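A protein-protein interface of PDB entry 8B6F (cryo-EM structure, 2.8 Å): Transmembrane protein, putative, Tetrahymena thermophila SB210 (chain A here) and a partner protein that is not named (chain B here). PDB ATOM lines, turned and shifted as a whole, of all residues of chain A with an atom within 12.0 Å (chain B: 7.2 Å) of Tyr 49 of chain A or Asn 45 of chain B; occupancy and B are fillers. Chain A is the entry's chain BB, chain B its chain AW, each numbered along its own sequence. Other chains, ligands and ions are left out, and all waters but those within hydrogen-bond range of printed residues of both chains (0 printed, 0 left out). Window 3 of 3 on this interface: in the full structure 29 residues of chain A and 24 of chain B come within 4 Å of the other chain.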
ATOM      1  N   GLY A  48     -24.076  11.354 -28.167  1.00  0.00           N
ATOM      2  CA  GLY A  48     -25.452  10.883 -27.851  1.00  0.00           C
ATOM      3  C   GLY A  48     -26.016  11.527 -26.601  1.00  0.00           C
ATOM      4  O   GLY A  48     -26.780  10.907 -25.861  1.00  0.00           O
ATOM      5  N   TYR A  49     -25.639  12.783 -26.365  1.00  0.00           N
ATOM      6  CA  TYR A  49     -26.088  13.532 -25.201  1.00  0.00           C
ATOM      7  C   TYR A  49     -27.283  14.425 -25.505  1.00  0.00           C
ATOM      8  O   TYR A  49     -27.688  15.211 -24.645  1.00  0.00           O
ATOM      9  CB  TYR A  49     -24.939  14.374 -24.644  1.00  0.00           C
ATOM     10  CG  TYR A  49     -23.788  13.565 -24.087  1.00  0.00           C
ATOM     11  CD1 TYR A  49     -24.014  12.387 -23.383  1.00  0.00           C
ATOM     12  CD2 TYR A  49     -22.475  13.978 -24.266  1.00  0.00           C
ATOM     13  CE1 TYR A  49     -22.966  11.647 -22.873  1.00  0.00           C
ATOM     14  CE2 TYR A  49     -21.420  13.243 -23.759  1.00  0.00           C
ATOM     15  CZ  TYR A  49     -21.673  12.079 -23.065  1.00  0.00           C
ATOM     16  OH  TYR A  49     -20.627  11.343 -22.559  1.00  0.00           O
ATOM     17  N   GLU A  50     -27.848  14.329 -26.706  1.00  0.00           N
ATOM     18  CA  GLU A  50     -29.037  15.105 -27.025  1.00  0.00           C
ATOM     19  C   GLU A  50     -30.200  14.657 -26.150  1.00  0.00           C
ATOM     20  O   GLU A  50     -30.356  13.468 -25.855  1.00  0.00           O
ATOM     21  CB  GLU A  50     -29.384  14.956 -28.508  1.00  0.00           C
ATOM     22  CG  GLU A  50     -29.647  13.523 -28.970  1.00  0.00           C
ATOM     23  CD  GLU A  50     -31.089  13.086 -28.782  1.00  0.00           C
ATOM     24  OE1 GLU A  50     -31.925  13.922 -28.380  1.00  0.00           O
ATOM     25  OE2 GLU A  50     -31.388  11.902 -29.046  1.00  0.00           O
ATOM     26  N   VAL A  51     -31.019  15.617 -25.730  1.00  0.00           N
ATOM     27  CA  VAL A  51     -32.119  15.377 -24.805  1.00  0.00           C
ATOM     28  C   VAL A  51     -33.433  15.466 -25.565  1.00  0.00           C
ATOM     29  O   VAL A  51     -33.629  16.367 -26.389  1.00  0.00           O
ATOM     30  CB  VAL A  51     -32.097  16.374 -23.629  1.00  0.00           C
ATOM     31  CG1 VAL A  51     -30.787  16.264 -22.867  1.00  0.00           C
ATOM     32  CG2 VAL A  51     -32.310  17.800 -24.123  1.00  0.00           C
ATOM     33  N   HIS A  52     -34.331  14.523 -25.291  1.00  0.00           N
ATOM     34  CA  HIS A  52     -35.662  14.511 -25.895  1.00  0.00           C
ATOM     35  C   HIS A  52     -36.566  15.403 -25.052  1.00  0.00           C
ATOM     36  O   HIS A  52     -37.084  14.981 -24.016  1.00  0.00           O
ATOM     37  CB  HIS A  52     -36.202  13.089 -25.980  1.00  0.00           C
ATOM     38  CG  HIS A  52     -37.589  13.002 -26.536  1.00  0.00           C
ATOM     39  ND1 HIS A  52     -38.706  13.356 -25.811  1.00  0.00           N
ATOM     40  CD2 HIS A  52     -38.039  12.595 -27.747  1.00  0.00           C
ATOM     41  CE1 HIS A  52     -39.784  13.174 -26.551  1.00  0.00           C
ATOM     42  NE2 HIS A  52     -39.408  12.713 -27.730  1.00  0.00           N
ATOM     43  N   LEU A  53     -36.757  16.643 -25.498  1.00  0.00           N
ATOM     44  CA  LEU A  53     -37.611  17.606 -24.816  1.00  0.00           C
ATOM     45  C   LEU A  53     -38.631  18.143 -25.806  1.00  0.00           C
ATOM     46  O   LEU A  53     -38.268  18.550 -26.914  1.00  0.00           O
ATOM     47  CB  LEU A  53     -36.787  18.752 -24.217  1.00  0.00           C
ATOM     48  CG  LEU A  53     -37.566  19.819 -23.443  1.00  0.00           C
ATOM     49  CD1 LEU A  53     -38.334  19.209 -22.279  1.00  0.00           C
ATOM     50  CD2 LEU A  53     -36.625  20.905 -22.945  1.00  0.00           C
ATOM     51  N   HIS A  81     -42.232  10.222 -23.885  1.00  0.00           N
ATOM     52  CA  HIS A  81     -41.173   9.324 -24.342  1.00  0.00           C
ATOM     53  C   HIS A  81     -41.021   8.216 -23.303  1.00  0.00           C
ATOM     54  O   HIS A  81     -40.152   8.249 -22.434  1.00  0.00           O
ATOM     55  CB  HIS A  81     -39.871  10.091 -24.551  1.00  0.00           C
ATOM     56  CG  HIS A  81     -38.700   9.216 -24.875  1.00  0.00           C
ATOM     57  ND1 HIS A  81     -37.401   9.574 -24.579  1.00  0.00           N
ATOM     58  CD2 HIS A  81     -38.629   8.004 -25.473  1.00  0.00           C
ATOM     59  CE1 HIS A  81     -36.582   8.618 -24.979  1.00  0.00           C
ATOM     60  NE2 HIS A  81     -37.302   7.654 -25.524  1.00  0.00           N
ATOM     61  N   GLU A 117     -16.594   1.553 -11.418  1.00  0.00           N
ATOM     62  CA  GLU A 117     -16.685   2.984 -11.167  1.00  0.00           C
ATOM     63  C   GLU A 117     -15.484   3.686 -11.789  1.00  0.00           C
ATOM     64  O   GLU A 117     -14.337   3.414 -11.421  1.00  0.00           O
ATOM     65  CB  GLU A 117     -16.748   3.254  -9.668  1.00  0.00           C
ATOM     66  CG  GLU A 117     -16.869   4.725  -9.309  1.00  0.00           C
ATOM     67  CD  GLU A 117     -18.154   5.350  -9.811  1.00  0.00           C
ATOM     68  OE1 GLU A 117     -19.082   4.597 -10.172  1.00  0.00           O
ATOM     69  OE2 GLU A 117     -18.236   6.596  -9.844  1.00  0.00           O
ATOM     70  N   GLY A 118     -15.748   4.590 -12.725  1.00  0.00           N
ATOM     71  CA  GLY A 118     -14.699   5.275 -13.448  1.00  0.00           C
ATOM     72  C   GLY A 118     -14.045   6.421 -12.718  1.00  0.00           C
ATOM     73  O   GLY A 118     -13.095   7.005 -13.242  1.00  0.00           O
ATOM     74  N   LEU A 119     -14.527   6.770 -11.523  1.00  0.00           N
ATOM     75  CA  LEU A 119     -13.965   7.870 -10.748  1.00  0.00           C
ATOM     76  C   LEU A 119     -13.332   7.411  -9.442  1.00  0.00           C
ATOM     77  O   LEU A 119     -12.968   8.255  -8.615  1.00  0.00           O
ATOM     78  CB  LEU A 119     -15.043   8.922 -10.471  1.00  0.00           C
ATOM     79  CG  LEU A 119     -15.470   9.746 -11.691  1.00  0.00           C
ATOM     80  CD1 LEU A 119     -16.709  10.560 -11.389  1.00  0.00           C
ATOM     81  CD2 LEU A 119     -14.347  10.659 -12.153  1.00  0.00           C
ATOM     82  N   VAL B  42      -7.891  12.557 -17.677  1.00  0.00           N
ATOM     83  CA  VAL B  42      -9.301  12.628 -18.035  1.00  0.00           C
ATOM     84  C   VAL B  42      -9.837  13.983 -17.597  1.00  0.00           C
ATOM     85  O   VAL B  42      -9.546  14.445 -16.489  1.00  0.00           O
ATOM     86  CB  VAL B  42     -10.112  11.484 -17.391  1.00  0.00           C
ATOM     87  CG1 VAL B  42     -11.568  11.546 -17.830  1.00  0.00           C
ATOM     88  CG2 VAL B  42      -9.502  10.136 -17.738  1.00  0.00           C
ATOM     89  N   LEU B  43     -10.618  14.614 -18.467  1.00  0.00           N
ATOM     90  CA  LEU B  43     -11.156  15.944 -18.226  1.00  0.00           C
ATOM     91  C   LEU B  43     -12.633  15.872 -17.856  1.00  0.00           C
ATOM     92  O   LEU B  43     -13.306  14.863 -18.076  1.00  0.00           O
ATOM     93  CB  LEU B  43     -10.973  16.829 -19.461  1.00  0.00           C
ATOM     94  CG  LEU B  43      -9.553  16.897 -20.025  1.00  0.00           C
ATOM     95  CD1 LEU B  43      -9.504  17.841 -21.213  1.00  0.00           C
ATOM     96  CD2 LEU B  43      -8.559  17.323 -18.959  1.00  0.00           C
ATOM     97  N   ARG B  44     -13.131  16.969 -17.289  1.00  0.00           N
ATOM     98  CA  ARG B  44     -14.534  17.044 -16.908  1.00  0.00           C
ATOM     99  C   ARG B  44     -15.422  16.794 -18.118  1.00  0.00           C
ATOM    100  O   ARG B  44     -15.193  17.348 -19.196  1.00  0.00           O
ATOM    101  CB  ARG B  44     -14.843  18.410 -16.298  1.00  0.00           C
ATOM    102  CG  ARG B  44     -14.106  18.684 -15.000  1.00  0.00           C
ATOM    103  CD  ARG B  44     -14.419  20.067 -14.449  1.00  0.00           C
ATOM    104  NE  ARG B  44     -15.839  20.247 -14.165  1.00  0.00           N
ATOM    105  CZ  ARG B  44     -16.723  20.752 -15.015  1.00  0.00           C
ATOM    106  NH1 ARG B  44     -16.372  21.142 -16.230  1.00  0.00           N
ATOM    107  NH2 ARG B  44     -17.993  20.868 -14.638  1.00  0.00           N
ATOM    108  N   ASN B  45     -16.440  15.962 -17.934  1.00  0.00           N
ATOM    109  CA  ASN B  45     -17.339  15.551 -19.010  1.00  0.00           C
ATOM    110  C   ASN B  45     -18.718  16.144 -18.733  1.00  0.00           C
ATOM    111  O   ASN B  45     -19.537  15.551 -18.031  1.00  0.00           O
ATOM    112  CB  ASN B  45     -17.396  14.031 -19.121  1.00  0.00           C
ATOM    113  CG  ASN B  45     -18.302  13.562 -20.241  1.00  0.00           C
ATOM    114  OD1 ASN B  45     -18.667  14.335 -21.123  1.00  0.00           O
ATOM    115  ND2 ASN B  45     -18.664  12.286 -20.211  1.00  0.00           N
ATOM    116  N   GLU B  46     -18.969  17.324 -19.300  1.00  0.00           N
ATOM    117  CA  GLU B  46     -20.280  17.965 -19.225  1.00  0.00           C
ATOM    118  C   GLU B  46     -21.168  17.327 -20.289  1.00  0.00           C
ATOM    119  O   GLU B  46     -21.337  17.834 -21.401  1.00  0.00           O
ATOM    120  CB  GLU B  46     -20.154  19.470 -19.414  1.00  0.00           C
ATOM    121  CG  GLU B  46     -19.247  20.136 -18.393  1.00  0.00           C
ATOM    122  CD  GLU B  46     -19.126  21.629 -18.608  1.00  0.00           C
ATOM    123  OE1 GLU B  46     -19.741  22.143 -19.565  1.00  0.00           O
ATOM    124  OE2 GLU B  46     -18.417  22.289 -17.821  1.00  0.00           O
ATOM    125  N   LYS B  47     -21.747  16.181 -19.929  1.00  0.00           N
ATOM    126  CA  LYS B  47     -22.535  15.406 -20.882  1.00  0.00           C
ATOM    127  C   LYS B  47     -23.649  16.253 -21.483  1.00  0.00           C
ATOM    128  O   LYS B  47     -23.669  16.522 -22.689  1.00  0.00           O
ATOM    129  CB  LYS B  47     -23.111  14.171 -20.187  1.00  0.00           C
ATOM    130  CG  LYS B  47     -22.070  13.292 -19.504  1.00  0.00           C
ATOM    131  CD  LYS B  47     -22.722  12.310 -18.545  1.00  0.00           C
ATOM    132  CE  LYS B  47     -21.685  11.491 -17.797  1.00  0.00           C
ATOM    133  NZ  LYS B  47     -20.952  10.559 -18.702  1.00  0.00           N
ATOM    134  N   SER B  48     -24.586  16.687 -20.648  1.00  0.00           N
ATOM    135  CA  SER B  48     -25.629  17.620 -21.038  1.00  0.00           C
ATOM    136  C   SER B  48     -25.892  18.537 -19.856  1.00  0.00           C
ATOM    137  O   SER B  48     -25.965  18.079 -18.714  1.00  0.00           O
ATOM    138  CB  SER B  48     -26.912  16.896 -21.464  1.00  0.00           C
ATOM    139  OG  SER B  48     -27.338  15.978 -20.473  1.00  0.00           O
ATOM    140  N   GLY B  49     -26.043  19.827 -20.133  1.00  0.00           N
ATOM    141  CA  GLY B  49     -26.178  20.819 -19.083  1.00  0.00           C
ATOM    142  C   GLY B  49     -27.195  20.467 -18.015  1.00  0.00           C
ATOM    143  O   GLY B  49     -27.124  20.982 -16.896  1.00  0.00           O
ATOM    144  N   TYR B  50     -28.142  19.594 -18.343  1.00  0.00           N
ATOM    145  CA  TYR B  50     -29.194  19.214 -17.411  1.00  0.00           C
ATOM    146  C   TYR B  50     -28.662  18.197 -16.409  1.00  0.00           C
ATOM    147  O   TYR B  50     -28.143  17.146 -16.798  1.00  0.00           O
ATOM    148  CB  TYR B  50     -30.384  18.635 -18.170  1.00  0.00           C
ATOM    149  CG  TYR B  50     -30.851  19.486 -19.325  1.00  0.00           C
ATOM    150  CD1 TYR B  50     -31.790  20.489 -19.139  1.00  0.00           C
ATOM    151  CD2 TYR B  50     -30.356  19.278 -20.605  1.00  0.00           C
ATOM    152  CE1 TYR B  50     -32.221  21.266 -20.195  1.00  0.00           C
ATOM    153  CE2 TYR B  50     -30.780  20.048 -21.666  1.00  0.00           C
ATOM    154  CZ  TYR B  50     -31.713  21.040 -21.456  1.00  0.00           C
ATOM    155  OH  TYR B  50     -32.138  21.812 -22.512  1.00  0.00           O
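The side-chain amide nitrogen (ND2) of Asn 45 of chain B lies close to the side-chain amino group (NZ) of Lys 47 of chain B, 3.2 Å away.
No residue of chain B comes within 4 Å of Gly 48 of chain A.
Of chain B, only Asn 45 (3.2 Å), Lys 47 (3.2 Å) and Ser 48 (3.7 Å) come within 4 Å of Tyr 49 of chain A.
Of the printed residues of chain B, Val 51 of chain A touches Tyr 50.
Glu 117 of chain A touches none of the printed residues of chain B.
Of chain A, only Tyr 49 comes within 4 Å of Asn 45 of chain B.
Glu 46 of chain B touches none of the printed residues of chain A.
Lys 47 of chain B touches just one residue of chain A: Tyr 49.
Gly 49 of chain B touches none of the printed residues of chain A.
Printed residues of chain A within 4 Å of Tyr 50 of chain B: Val 51 (3.7 Å).
The nearest residue of chain B that does not touch Tyr 49 of chain A is Glu 46 of chain B (4.9 Å).
The nearest printed residue of chain A that does not touch Tyr 50 of chain B is Leu 53 of chain A (4.6 Å).
OH of Tyr 49 of chain A lies within hydrogen-bond range of ND2 of Asn 45 of chain B (3.2 Å).
Among the printed residues, pairs that only touch across the chains: Tyr 49 of chain A with Lys 47 of chain B (3.2 Å), Tyr 49 of chain A with Ser 48 of chain B (3.7 Å) and Val 51 of chain A with Tyr 50 of chain B (3.7 Å).
Hydrophobic or aromatic side chains of chain B within 4 Å of the printed part of chain A: Tyr 50.
Among the printed residues, 4 pairs touch across the chains.
Among the printed residues, no Asp or Glu carboxylate lies within 4 Å of a Lys or Arg side-chain nitrogen of the other chain.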
